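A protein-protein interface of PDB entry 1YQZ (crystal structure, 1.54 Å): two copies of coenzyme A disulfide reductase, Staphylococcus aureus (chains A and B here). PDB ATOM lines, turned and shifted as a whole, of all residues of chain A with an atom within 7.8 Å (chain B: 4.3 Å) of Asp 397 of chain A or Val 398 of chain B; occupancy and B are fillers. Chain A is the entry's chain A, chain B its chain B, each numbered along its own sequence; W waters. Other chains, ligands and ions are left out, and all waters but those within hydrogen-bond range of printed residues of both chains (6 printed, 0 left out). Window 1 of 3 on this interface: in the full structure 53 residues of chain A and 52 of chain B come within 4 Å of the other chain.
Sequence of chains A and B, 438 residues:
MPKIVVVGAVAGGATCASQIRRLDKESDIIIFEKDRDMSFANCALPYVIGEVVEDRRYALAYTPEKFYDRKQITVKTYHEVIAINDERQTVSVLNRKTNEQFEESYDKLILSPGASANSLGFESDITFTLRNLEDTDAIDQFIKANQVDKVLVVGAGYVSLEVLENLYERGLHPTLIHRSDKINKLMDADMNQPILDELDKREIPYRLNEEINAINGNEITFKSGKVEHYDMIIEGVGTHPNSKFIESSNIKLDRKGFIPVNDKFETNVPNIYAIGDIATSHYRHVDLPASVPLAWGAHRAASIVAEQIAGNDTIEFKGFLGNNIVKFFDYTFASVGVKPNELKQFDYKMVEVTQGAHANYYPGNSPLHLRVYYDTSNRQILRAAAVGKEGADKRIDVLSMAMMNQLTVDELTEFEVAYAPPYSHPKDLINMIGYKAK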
ATOM      1  N   LEU A 321      28.580   4.282  24.972  1.00  0.00           N
ATOM      2  CA  LEU A 321      28.910   4.163  23.548  1.00  0.00           C
ATOM      3  C   LEU A 321      29.797   5.362  23.174  1.00  0.00           C
ATOM      4  O   LEU A 321      30.537   5.311  22.172  1.00  0.00           O
ATOM      5  CB  LEU A 321      27.660   4.143  22.661  1.00  0.00           C
ATOM      6  CG  LEU A 321      26.882   2.820  22.771  1.00  0.00           C
ATOM      7  CD1 LEU A 321      25.593   2.936  21.993  1.00  0.00           C
ATOM      8  CD2 LEU A 321      27.705   1.659  22.211  1.00  0.00           C
ATOM      9  N   ASN A 323      28.666   8.620  22.495  1.00  0.00           N
ATOM     10  CA  ASN A 323      28.078   9.473  21.466  1.00  0.00           C
ATOM     11  C   ASN A 323      28.369  10.919  21.844  1.00  0.00           C
ATOM     12  O   ASN A 323      28.163  11.322  22.996  1.00  0.00           O
ATOM     13  CB  ASN A 323      26.567   9.224  21.370  1.00  0.00           C
ATOM     14  CG  ASN A 323      25.990   9.663  20.037  1.00  0.00           C
ATOM     15  OD1 ASN A 323      26.681  10.314  19.235  1.00  0.00           O
ATOM     16  ND2 ASN A 323      24.717   9.323  19.792  1.00  0.00           N
ATOM     17  N   ASN A 324      28.874  11.684  20.881  1.00  0.00           N
ATOM     18  CA  ASN A 324      29.222  13.091  21.109  1.00  0.00           C
ATOM     19  C   ASN A 324      29.055  13.929  19.852  1.00  0.00           C
ATOM     20  O   ASN A 324      29.076  13.418  18.709  1.00  0.00           O
ATOM     21  CB  ASN A 324      30.659  13.173  21.601  1.00  0.00           C
ATOM     22  CG  ASN A 324      31.652  12.779  20.518  1.00  0.00           C
ATOM     23  OD1 ASN A 324      32.186  13.626  19.801  1.00  0.00           O
ATOM     24  ND2 ASN A 324      31.867  11.481  20.362  1.00  0.00           N
ATOM     25  N   ILE A 325      28.921  15.241  20.036  1.00  0.00           N
ATOM     26  CA  ILE A 325      28.681  16.083  18.873  1.00  0.00           C
ATOM     27  C   ILE A 325      28.975  17.533  19.208  1.00  0.00           C
ATOM     28  O   ILE A 325      28.934  17.937  20.387  1.00  0.00           O
ATOM     29  CB  ILE A 325      27.169  15.926  18.472  1.00  0.00           C
ATOM     30  CG1 ILE A 325      26.839  16.695  17.198  1.00  0.00           C
ATOM     31  CG2 ILE A 325      26.271  16.497  19.591  1.00  0.00           C
ATOM     32  CD1 ILE A 325      25.496  16.253  16.601  1.00  0.00           C
ATOM     33  N   ALA A 334      29.996  14.772  14.533  1.00  0.00           N
ATOM     34  CA  ALA A 334      29.462  13.832  15.506  1.00  0.00           C
ATOM     35  C   ALA A 334      30.115  12.461  15.366  1.00  0.00           C
ATOM     36  O   ALA A 334      30.435  12.039  14.262  1.00  0.00           O
ATOM     37  CB  ALA A 334      27.941  13.692  15.297  1.00  0.00           C
ATOM     38  N   SER A 335      30.346  11.798  16.497  1.00  0.00           N
ATOM     39  CA  SER A 335      30.901  10.451  16.453  1.00  0.00           C
ATOM     40  C   SER A 335      30.398   9.625  17.618  1.00  0.00           C
ATOM     41  O   SER A 335      29.871  10.155  18.604  1.00  0.00           O
ATOM     42  CB  SER A 335      32.429  10.453  16.432  1.00  0.00           C
ATOM     43  OG  SER A 335      33.000  10.924  17.643  1.00  0.00           O
ATOM     44  N   VAL A 336      30.531   8.315  17.476  1.00  0.00           N
ATOM     45  CA  VAL A 336      30.079   7.388  18.509  1.00  0.00           C
ATOM     46  C   VAL A 336      30.933   6.127  18.464  1.00  0.00           C
ATOM     47  O   VAL A 336      31.431   5.750  17.396  1.00  0.00           O
ATOM     48  CB  VAL A 336      28.573   7.056  18.332  1.00  0.00           C
ATOM     49  CG1 VAL A 336      28.278   6.429  16.938  1.00  0.00           C
ATOM     50  CG2 VAL A 336      28.106   6.165  19.457  1.00  0.00           C
ATOM     51  N   ALA A 386      30.453  11.310  11.507  1.00  0.00           N
ATOM     52  CA  ALA A 386      29.785  12.005  10.416  1.00  0.00           C
ATOM     53  C   ALA A 386      30.041  13.490  10.516  1.00  0.00           C
ATOM     54  O   ALA A 386      30.023  14.054  11.602  1.00  0.00           O
ATOM     55  CB  ALA A 386      28.279  11.728  10.439  1.00  0.00           C
ATOM     56  N   GLY A 391      22.352  16.771   8.495  1.00  0.00           N
ATOM     57  CA  GLY A 391      22.161  15.331   8.648  1.00  0.00           C
ATOM     58  C   GLY A 391      23.110  14.465   9.439  1.00  0.00           C
ATOM     59  O   GLY A 391      22.829  13.267   9.635  1.00  0.00           O
ATOM     60  N   ALA A 392      24.199  15.043   9.923  1.00  0.00           N
ATOM     61  CA  ALA A 392      25.169  14.246  10.666  1.00  0.00           C
ATOM     62  C   ALA A 392      24.615  13.765  12.000  1.00  0.00           C
ATOM     63  O   ALA A 392      24.848  12.612  12.391  1.00  0.00           O
ATOM     64  CB  ALA A 392      26.460  15.049  10.884  1.00  0.00           C
ATOM     65  N   ASP A 393      23.878  14.618  12.710  1.00  0.00           N
ATOM     66  CA  ASP A 393      23.312  14.186  13.971  1.00  0.00           C
ATOM     67  C   ASP A 393      22.324  13.023  13.775  1.00  0.00           C
ATOM     68  O   ASP A 393      22.296  12.063  14.557  1.00  0.00           O
ATOM     69  CB  ASP A 393      22.629  15.353  14.733  1.00  0.00           C
ATOM     70  CG  ASP A 393      21.602  16.098  13.902  1.00  0.00           C
ATOM     71  OD1 ASP A 393      20.605  16.566  14.499  1.00  0.00           O
ATOM     72  OD2 ASP A 393      21.786  16.231  12.675  1.00  0.00           O
ATOM     73  N   LYS A 394      21.523  13.097  12.720  1.00  0.00           N
ATOM     74  CA  LYS A 394      20.568  12.018  12.481  1.00  0.00           C
ATOM     75  C   LYS A 394      21.262  10.669  12.212  1.00  0.00           C
ATOM     76  O   LYS A 394      20.880   9.636  12.785  1.00  0.00           O
ATOM     77  CB  LYS A 394      19.659  12.373  11.294  1.00  0.00           C
ATOM     78  CG  LYS A 394      18.674  11.257  10.931  1.00  0.00           C
ATOM     79  CD  LYS A 394      17.536  11.777  10.034  1.00  0.00           C
ATOM     80  CE  LYS A 394      18.058  12.237   8.681  1.00  0.00           C
ATOM     81  NZ  LYS A 394      16.912  12.656   7.789  1.00  0.00           N
ATOM     82  N   ARG A 395      22.307  10.676  11.390  1.00  0.00           N
ATOM     83  CA  ARG A 395      22.942   9.413  11.066  1.00  0.00           C
ATOM     84  C   ARG A 395      23.668   8.826  12.265  1.00  0.00           C
ATOM     85  O   ARG A 395      23.643   7.617  12.474  1.00  0.00           O
ATOM     86  CB  ARG A 395      23.960   9.540   9.916  1.00  0.00           C
ATOM     87  CG  ARG A 395      23.429  10.077   8.571  1.00  0.00           C
ATOM     88  CD  ARG A 395      21.986   9.678   8.327  1.00  0.00           C
ATOM     89  NE  ARG A 395      21.458   9.929   6.967  1.00  0.00           N
ATOM     90  CZ  ARG A 395      21.036  11.106   6.498  1.00  0.00           C
ATOM     91  NH1 ARG A 395      20.533  11.183   5.259  1.00  0.00           N
ATOM     92  NH2 ARG A 395      21.154  12.222   7.204  1.00  0.00           N
ATOM     93  N   ILE A 396      24.307   9.690  13.048  1.00  0.00           N
ATOM     94  CA  ILE A 396      25.060   9.175  14.190  1.00  0.00           C
ATOM     95  C   ILE A 396      24.115   8.668  15.300  1.00  0.00           C
ATOM     96  O   ILE A 396      24.429   7.682  15.962  1.00  0.00           O
ATOM     97  CB  ILE A 396      26.097  10.239  14.686  1.00  0.00           C
ATOM     98  CG1 ILE A 396      27.211  10.378  13.630  1.00  0.00           C
ATOM     99  CG2 ILE A 396      26.754   9.801  16.004  1.00  0.00           C
ATOM    100  CD1 ILE A 396      27.972   9.049  13.344  1.00  0.00           C
ATOM    101  N   ASP A 397      22.961   9.303  15.496  1.00  0.00           N
ATOM    102  CA  ASP A 397      22.014   8.795  16.496  1.00  0.00           C
ATOM    103  C   ASP A 397      21.455   7.450  16.038  1.00  0.00           C
ATOM    104  O   ASP A 397      21.242   6.541  16.848  1.00  0.00           O
ATOM    105  CB  ASP A 397      20.865   9.777  16.722  1.00  0.00           C
ATOM    106  CG  ASP A 397      21.193  10.816  17.788  1.00  0.00           C
ATOM    107  OD1 ASP A 397      22.250  10.680  18.470  1.00  0.00           O
ATOM    108  OD2 ASP A 397      20.376  11.737  17.964  1.00  0.00           O
ATOM    109  N   VAL A 398      21.203   7.294  14.734  1.00  0.00           N
ATOM    110  CA  VAL A 398      20.709   5.995  14.270  1.00  0.00           C
ATOM    111  C   VAL A 398      21.786   4.923  14.516  1.00  0.00           C
ATOM    112  O   VAL A 398      21.479   3.807  14.944  1.00  0.00           O
ATOM    113  CB  VAL A 398      20.349   6.054  12.746  1.00  0.00           C
ATOM    114  CG1 VAL A 398      20.135   4.669  12.182  1.00  0.00           C
ATOM    115  CG2 VAL A 398      19.097   6.876  12.540  1.00  0.00           C
ATOM    116  N   LEU A 399      23.057   5.256  14.266  1.00  0.00           N
ATOM    117  CA  LEU A 399      24.122   4.272  14.459  1.00  0.00           C
ATOM    118  C   LEU A 399      24.355   3.988  15.941  1.00  0.00           C
ATOM    119  O   LEU A 399      24.721   2.878  16.313  1.00  0.00           O
ATOM    120  CB  LEU A 399      25.402   4.721  13.744  1.00  0.00           C
ATOM    121  CG  LEU A 399      25.222   4.631  12.217  1.00  0.00           C
ATOM    122  CD1 LEU A 399      26.399   5.305  11.511  1.00  0.00           C
ATOM    123  CD2 LEU A 399      25.132   3.163  11.780  1.00  0.00           C
ATOM    124  N   SER A 400      24.141   4.986  16.798  1.00  0.00           N
ATOM    125  CA  SER A 400      24.241   4.725  18.234  1.00  0.00           C
ATOM    126  C   SER A 400      23.186   3.660  18.605  1.00  0.00           C
ATOM    127  O   SER A 400      23.474   2.726  19.353  1.00  0.00           O
ATOM    128  CB  SER A 400      23.970   6.011  19.029  1.00  0.00           C
ATOM    129  OG  SER A 400      23.971   5.725  20.420  1.00  0.00           O
ATOM    130  N   MET A 401      21.954   3.802  18.094  1.00  0.00           N
ATOM    131  CA  MET A 401      20.914   2.833  18.385  1.00  0.00           C
ATOM    132  C   MET A 401      21.285   1.454  17.827  1.00  0.00           C
ATOM    133  O   MET A 401      20.996   0.420  18.441  1.00  0.00           O
ATOM    134  CB  MET A 401      19.586   3.326  17.804  1.00  0.00           C
ATOM    135  CG  MET A 401      18.419   2.340  17.943  1.00  0.00           C
ATOM    136  SD  MET A 401      18.025   1.888  19.671  1.00  0.00           S
ATOM    137  CE  MET A 401      17.211   3.369  20.231  1.00  0.00           C
ATOM    138  N   ALA A 402      21.932   1.432  16.663  1.00  0.00           N
ATOM    139  CA  ALA A 402      22.337   0.157  16.073  1.00  0.00           C
ATOM    140  C   ALA A 402      23.408  -0.493  16.951  1.00  0.00           C
ATOM    141  O   ALA A 402      23.366  -1.701  17.215  1.00  0.00           O
ATOM    142  CB  ALA A 402      22.881   0.385  14.661  1.00  0.00           C
ATOM    143  N   MET A 403      24.369   0.302  17.421  1.00  0.00           N
ATOM    144  CA  MET A 403      25.452  -0.239  18.247  1.00  0.00           C
ATOM    145  C   MET A 403      24.958  -0.738  19.606  1.00  0.00           C
ATOM    146  O   MET A 403      25.469  -1.727  20.155  1.00  0.00           O
ATOM    147  CB  MET A 403      26.534   0.825  18.418  1.00  0.00           C
ATOM    148  CG  MET A 403      27.260   1.088  17.127  1.00  0.00           C
ATOM    149  SD  MET A 403      28.102   2.666  17.149  1.00  0.00           S
ATOM    150  CE  MET A 403      29.610   2.186  17.946  1.00  0.00           C
ATOM    151  N   MET A 404      23.946  -0.059  20.135  1.00  0.00           N
ATOM    152  CA  MET A 404      23.368  -0.424  21.426  1.00  0.00           C
ATOM    153  C   MET A 404      23.003  -1.887  21.359  1.00  0.00           C
ATOM    154  O   MET A 404      23.001  -2.604  22.364  1.00  0.00           O
ATOM    155  CB  MET A 404      22.121   0.421  21.659  1.00  0.00           C
ATOM    156  CG  MET A 404      21.438   0.264  22.978  1.00  0.00           C
ATOM    157  SD  MET A 404      19.999   1.374  22.934  1.00  0.00           S
ATOM    158  CE  MET A 404      18.757   0.268  23.587  1.00  0.00           C
ATOM    159  N   ASN A 405      22.727  -2.327  20.146  1.00  0.00           N
ATOM    160  CA  ASN A 405      22.349  -3.696  19.902  1.00  0.00           C
ATOM    161  C   ASN A 405      23.448  -4.503  19.178  1.00  0.00           C
ATOM    162  O   ASN A 405      23.165  -5.556  18.607  1.00  0.00           O
ATOM    163  CB  ASN A 405      21.048  -3.670  19.111  1.00  0.00           C
ATOM    164  CG  ASN A 405      19.906  -3.049  19.901  1.00  0.00           C
ATOM    165  OD1 ASN A 405      19.547  -3.547  20.968  1.00  0.00           O
ATOM    166  ND2 ASN A 405      19.333  -1.958  19.388  1.00  0.00           N
ATOM    167  N   PHE A 415      18.247  -1.186   7.226  1.00  0.00           N
ATOM    168  CA  PHE A 415      17.697  -0.038   7.921  1.00  0.00           C
ATOM    169  C   PHE A 415      16.656   0.627   7.021  1.00  0.00           C
ATOM    170  O   PHE A 415      16.944   0.950   5.867  1.00  0.00           O
ATOM    171  CB  PHE A 415      18.831   0.940   8.267  1.00  0.00           C
ATOM    172  CG  PHE A 415      18.351   2.304   8.665  1.00  0.00           C
ATOM    173  CD1 PHE A 415      17.509   2.469   9.763  1.00  0.00           C
ATOM    174  CD2 PHE A 415      18.734   3.416   7.932  1.00  0.00           C
ATOM    175  CE1 PHE A 415      17.056   3.755  10.115  1.00  0.00           C
ATOM    176  CE2 PHE A 415      18.293   4.703   8.270  1.00  0.00           C
ATOM    177  CZ  PHE A 415      17.455   4.861   9.357  1.00  0.00           C
ATOM    178  N   GLU A 416      15.456   0.840   7.560  1.00  0.00           N
ATOM    179  CA  GLU A 416      14.366   1.424   6.790  1.00  0.00           C
ATOM    180  C   GLU A 416      14.266   2.892   7.178  1.00  0.00           C
ATOM    181  O   GLU A 416      13.729   3.243   8.219  1.00  0.00           O
ATOM    182  CB  GLU A 416      13.067   0.649   7.095  1.00  0.00           C
ATOM    183  CG  GLU A 416      11.899   1.094   6.227  1.00  0.00           C
ATOM    184  CD  GLU A 416      10.664   0.236   6.383  1.00  0.00           C
ATOM    185  OE1 GLU A 416       9.565   0.789   6.185  1.00  0.00           O
ATOM    186  OE2 GLU A 416      10.776  -0.967   6.669  1.00  0.00           O
ATOM    187  N   ILE A 430      23.256   5.509   5.348  1.00  0.00           N
ATOM    188  CA  ILE A 430      23.430   4.365   6.238  1.00  0.00           C
ATOM    189  C   ILE A 430      23.302   3.040   5.462  1.00  0.00           C
ATOM    190  O   ILE A 430      24.093   2.103   5.650  1.00  0.00           O
ATOM    191  CB  ILE A 430      22.424   4.459   7.417  1.00  0.00           C
ATOM    192  CG1 ILE A 430      22.899   5.553   8.390  1.00  0.00           C
ATOM    193  CG2 ILE A 430      22.320   3.133   8.164  1.00  0.00           C
ATOM    194  CD1 ILE A 430      21.961   5.820   9.542  1.00  0.00           C
ATOM    195  N   LYS B 394      14.760  12.733  12.634  1.00  0.00           N
ATOM    196  CA  LYS B 394      15.798  12.098  13.429  1.00  0.00           C
ATOM    197  C   LYS B 394      15.179  11.124  14.439  1.00  0.00           C
ATOM    198  O   LYS B 394      15.630   9.983  14.552  1.00  0.00           O
ATOM    199  CB  LYS B 394      16.633  13.150  14.158  1.00  0.00           C
ATOM    200  CG  LYS B 394      17.750  12.528  15.041  1.00  0.00           C
ATOM    201  CD  LYS B 394      18.822  13.564  15.456  1.00  0.00           C
ATOM    202  CE  LYS B 394      18.261  14.644  16.366  1.00  0.00           C
ATOM    203  NZ  LYS B 394      19.319  15.630  16.774  1.00  0.00           N
ATOM    204  N   ARG B 395      14.142  11.559  15.164  1.00  0.00           N
ATOM    205  CA  ARG B 395      13.541  10.678  16.159  1.00  0.00           C
ATOM    206  C   ARG B 395      12.897   9.456  15.524  1.00  0.00           C
ATOM    207  O   ARG B 395      13.027   8.354  16.033  1.00  0.00           O
ATOM    208  CB  ARG B 395      12.490  11.403  17.019  1.00  0.00           C
ATOM    209  CG  ARG B 395      12.964  12.568  17.899  1.00  0.00           C
ATOM    210  CD  ARG B 395      14.445  12.550  18.158  1.00  0.00           C
ATOM    211  NE  ARG B 395      14.933  13.582  19.090  1.00  0.00           N
ATOM    212  CZ  ARG B 395      15.243  14.836  18.767  1.00  0.00           C
ATOM    213  NH1 ARG B 395      15.723  15.649  19.705  1.00  0.00           N
ATOM    214  NH2 ARG B 395      15.061  15.311  17.541  1.00  0.00           N
ATOM    215  N   ILE B 396      12.221   9.634  14.393  1.00  0.00           N
ATOM    216  CA  ILE B 396      11.589   8.459  13.784  1.00  0.00           C
ATOM    217  C   ILE B 396      12.598   7.469  13.174  1.00  0.00           C
ATOM    218  O   ILE B 396      12.389   6.249  13.277  1.00  0.00           O
ATOM    219  CB  ILE B 396      10.496   8.882  12.771  1.00  0.00           C
ATOM    220  CG1 ILE B 396       9.367   9.593  13.527  1.00  0.00           C
ATOM    221  CG2 ILE B 396       9.872   7.617  12.120  1.00  0.00           C
ATOM    222  CD1 ILE B 396       8.675   8.686  14.566  1.00  0.00           C
ATOM    223  N   ASP B 397      13.701   7.956  12.586  1.00  0.00           N
ATOM    224  CA  ASP B 397      14.702   7.015  12.069  1.00  0.00           C
ATOM    225  C   ASP B 397      15.350   6.232  13.240  1.00  0.00           C
ATOM    226  O   ASP B 397      15.666   5.056  13.112  1.00  0.00           O
ATOM    227  CB  ASP B 397      15.793   7.738  11.280  1.00  0.00           C
ATOM    228  CG  ASP B 397      15.396   8.019   9.840  1.00  0.00           C
ATOM    229  OD1 ASP B 397      14.370   7.480   9.377  1.00  0.00           O
ATOM    230  OD2 ASP B 397      16.128   8.769   9.164  1.00  0.00           O
ATOM    231  N   VAL B 398      15.566   6.895  14.381  1.00  0.00           N
ATOM    232  CA  VAL B 398      16.138   6.181  15.521  1.00  0.00           C
ATOM    233  C   VAL B 398      15.169   5.100  15.988  1.00  0.00           C
ATOM    234  O   VAL B 398      15.568   3.964  16.282  1.00  0.00           O
ATOM    235  CB  VAL B 398      16.445   7.134  16.702  1.00  0.00           C
ATOM    236  CG1 VAL B 398      16.746   6.325  17.973  1.00  0.00           C
ATOM    237  CG2 VAL B 398      17.627   8.037  16.333  1.00  0.00           C
ATOM    238  N   LEU B 399      13.877   5.434  16.017  1.00  0.00           N
ATOM    239  CA  LEU B 399      12.894   4.449  16.459  1.00  0.00           C
ATOM    240  C   LEU B 399      12.730   3.331  15.423  1.00  0.00           C
ATOM    241  O   LEU B 399      12.459   2.205  15.802  1.00  0.00           O
ATOM    242  CB  LEU B 399      11.579   5.130  16.800  1.00  0.00           C
ATOM    243  CG  LEU B 399      11.747   5.954  18.085  1.00  0.00           C
ATOM    244  CD1 LEU B 399      10.545   6.881  18.235  1.00  0.00           C
ATOM    245  CD2 LEU B 399      11.841   5.039  19.306  1.00  0.00           C
ATOM    246  N   SER B 400      12.913   3.638  14.137  1.00  0.00           N
ATOM    247  CA  SER B 400      12.877   2.576  13.123  1.00  0.00           C
ATOM    248  C   SER B 400      14.017   1.568  13.423  1.00  0.00           C
ATOM    249  O   SER B 400      13.819   0.338  13.384  1.00  0.00           O
ATOM    250  CB  SER B 400      13.048   3.178  11.722  1.00  0.00           C
ATOM    251  OG  SER B 400      13.119   2.142  10.742  1.00  0.00           O
ATOM    252  N   MET B 401      15.210   2.079  13.745  1.00  0.00           N
ATOM    253  CA  MET B 401      16.338   1.203  14.074  1.00  0.00           C
ATOM    254  C   MET B 401      16.053   0.429  15.366  1.00  0.00           C
ATOM    255  O   MET B 401      16.445  -0.740  15.490  1.00  0.00           O
ATOM    256  CB  MET B 401      17.620   2.034  14.187  1.00  0.00           C
ATOM    257  CG  MET B 401      18.858   1.237  14.572  1.00  0.00           C
ATOM    258  SD  MET B 401      19.307  -0.054  13.414  1.00  0.00           S
ATOM    259  CE  MET B 401      20.053   0.922  12.147  1.00  0.00           C
ATOM    260  N   ALA B 402      15.383   1.066  16.330  1.00  0.00           N
ATOM    261  CA  ALA B 402      15.051   0.369  17.565  1.00  0.00           C
ATOM    262  C   ALA B 402      14.113  -0.790  17.270  1.00  0.00           C
ATOM    263  O   ALA B 402      14.292  -1.884  17.787  1.00  0.00           O
ATOM    264  CB  ALA B 402      14.380   1.321  18.557  1.00  0.00           C
ATOM    265  N   PHE B 415      19.014   4.605  25.306  1.00  0.00           N
ATOM    266  CA  PHE B 415      19.494   5.179  24.057  1.00  0.00           C
ATOM    267  C   PHE B 415      20.431   6.356  24.379  1.00  0.00           C
ATOM    268  O   PHE B 415      20.055   7.311  25.059  1.00  0.00           O
ATOM    269  CB  PHE B 415      18.292   5.652  23.219  1.00  0.00           C
ATOM    270  CG  PHE B 415      18.651   6.609  22.111  1.00  0.00           C
ATOM    271  CD1 PHE B 415      19.540   6.232  21.096  1.00  0.00           C
ATOM    272  CD2 PHE B 415      18.123   7.906  22.098  1.00  0.00           C
ATOM    273  CE1 PHE B 415      19.893   7.147  20.088  1.00  0.00           C
ATOM    274  CE2 PHE B 415      18.475   8.826  21.085  1.00  0.00           C
ATOM    275  CZ  PHE B 415      19.367   8.430  20.080  1.00  0.00           C
ATOM    276  N   VAL B 417      21.965   9.414  23.152  1.00  0.00           N
ATOM    277  CA  VAL B 417      21.819  10.446  22.134  1.00  0.00           C
ATOM    278  C   VAL B 417      23.071  11.306  21.980  1.00  0.00           C
ATOM    279  O   VAL B 417      23.891  11.384  22.904  1.00  0.00           O
ATOM    280  CB  VAL B 417      20.635  11.374  22.513  1.00  0.00           C
ATOM    281  CG1 VAL B 417      21.037  12.261  23.697  1.00  0.00           C
ATOM    282  CG2 VAL B 417      20.212  12.236  21.301  1.00  0.00           C
ATOM    283  N   ALA B 418      23.219  11.936  20.815  1.00  0.00           N
ATOM    284  CA  ALA B 418      24.325  12.856  20.598  1.00  0.00           C
ATOM    285  C   ALA B 418      23.792  14.192  21.104  1.00  0.00           C
ATOM    286  O   ALA B 418      22.881  14.789  20.502  1.00  0.00           O
ATOM    287  CB  ALA B 418      24.675  12.953  19.119  1.00  0.00           C
ATOM    288  N   ILE B 430      13.399  10.742  23.038  1.00  0.00           N
ATOM    289  CA  ILE B 430      13.348   9.299  23.003  1.00  0.00           C
ATOM    290  C   ILE B 430      13.575   8.686  24.388  1.00  0.00           C
ATOM    291  O   ILE B 430      12.902   7.730  24.761  1.00  0.00           O
ATOM    292  CB  ILE B 430      14.364   8.738  21.979  1.00  0.00           C
ATOM    293  CG1 ILE B 430      13.843   9.057  20.568  1.00  0.00           C
ATOM    294  CG2 ILE B 430      14.536   7.219  22.149  1.00  0.00           C
ATOM    295  CD1 ILE B 430      14.823   8.711  19.467  1.00  0.00           C
HETATM  296  O   HOH W   1      17.634  11.868  18.591  1.00  0.00           O
HETATM  297  O   HOH W   2      18.867   8.690   8.508  1.00  0.00           O
HETATM  298  O   HOH W   3      21.195  14.293  18.363  1.00  0.00           O
HETATM  299  O   HOH W   4      26.030  12.815  23.788  1.00  0.00           O
HETATM  300  O   HOH W   5      15.173  10.570   7.431  1.00  0.00           O
HETATM  301  O   HOH W   6      15.088   0.098  10.280  1.00  0.00           O
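Ile 325 of chain A touches Ala 418 of chain B. CD of Lys 394 of chain B touches CA of Lys 394 of chain A, at 3.8 Å. CB of Asp 397 of chain A touches CG2 of Val 398 of chain B, at 3.7 Å. Val 398 of chain B touches Met 401 of chain A (O to CG, 3.7 Å). Asp 397 of chain B touches Phe 415 of chain A.
NZ of Lys 394 of chain B lies within salt-bridge range of OD1 of Asp 393 of chain A (2.8 Å). The backbone carbonyl oxygen (O) of Glu 416 of chain A is in hydrogen-bond range of the side-chain hydroxyl (OG) of Ser 400 of chain B (2.8 Å). ND2 of Asn 323 of chain A lies close to N of Ala 418 of chain B (3.2 Å). The backbone NH (N) of Ala 418 of chain B lies within hydrogen-bond range of the side-chain carboxylate (OD1) of Asp 397 of chain A, 2.8 Å away.
Of the 13 printed residues of chain B, 9 touch a printed residue of chain A. Hydrophobic or aromatic side chains of chain B that line the printed part of chain A: Val 398, Met 401, Ala 402, Phe 415, Val 417 and Ala 418. Printed residues of chain A that touch a printed residue of chain B: Asn 323, Ile 325, Asp 393, Lys 394, Asp 397, Val 398, Met 401, Ala 402, Met 404, Phe 415 and Glu 416. Hydrophobic or aromatic side chains of chain A that line the printed part of chain B: Ile 325, Val 398, Met 401, Ala 402, Met 404 and Phe 415. Among the printed residues, Asp or Glu carboxylates within 4 Å of a Lys or Arg side-chain nitrogen of the other chain: Asp 393 of chain A with Lys 394 of chain B.
Asp 397 of chain A touches Val 398 of chain B, and with the chains exchanged Val 398 of chain A touches Asp 397 of chain B. Val 398 of chain B touches its own counterpart, Val 398 of chain A. Met 401 of chain A touches Phe 415 of chain B, and with the chains exchanged Phe 415 of chain A touches Met 401 of chain B.
OD1 of Asn 323 of chain A lies close to O of Ser 335 of chain A (3.3 Å). The side-chain carboxylate (OD1) of Asp 397 of chain A lies within hydrogen-bond range of the side-chain amide nitrogen (ND2) of Asn 323 of chain A.
Leu 321 of chain A touches none of the printed residues of chain B. Printed residues of chain B within 4 Å of Glu 416 of chain A: Ser 400. Of the printed residues of chain A, Val 398 of chain B touches Asp 397 (3.7 Å), Val 398 (3.98 Å) and Met 401 (3.7 Å). The nearest printed residue of chain B that does not touch Asp 397 of chain A is Arg 395 of chain B (5.9 Å). The nearest printed residue of chain B that does not touch Lys 394 of chain A is Val 398 of chain B (5.1 Å).
Water W3 lies within hydrogen-bond range of OD2 of Asp 397 of chain A (2.7 Å), O of Ala 418 of chain B (2.8 Å) and NZ of Lys 394 of chain B (2.8 Å). Water W6 lies within hydrogen-bond range of the backbone NH (N) of Glu 416 of chain A (2.8 Å) and the side-chain hydroxyl (OG) of Ser 400 of chain B (2.9 Å).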
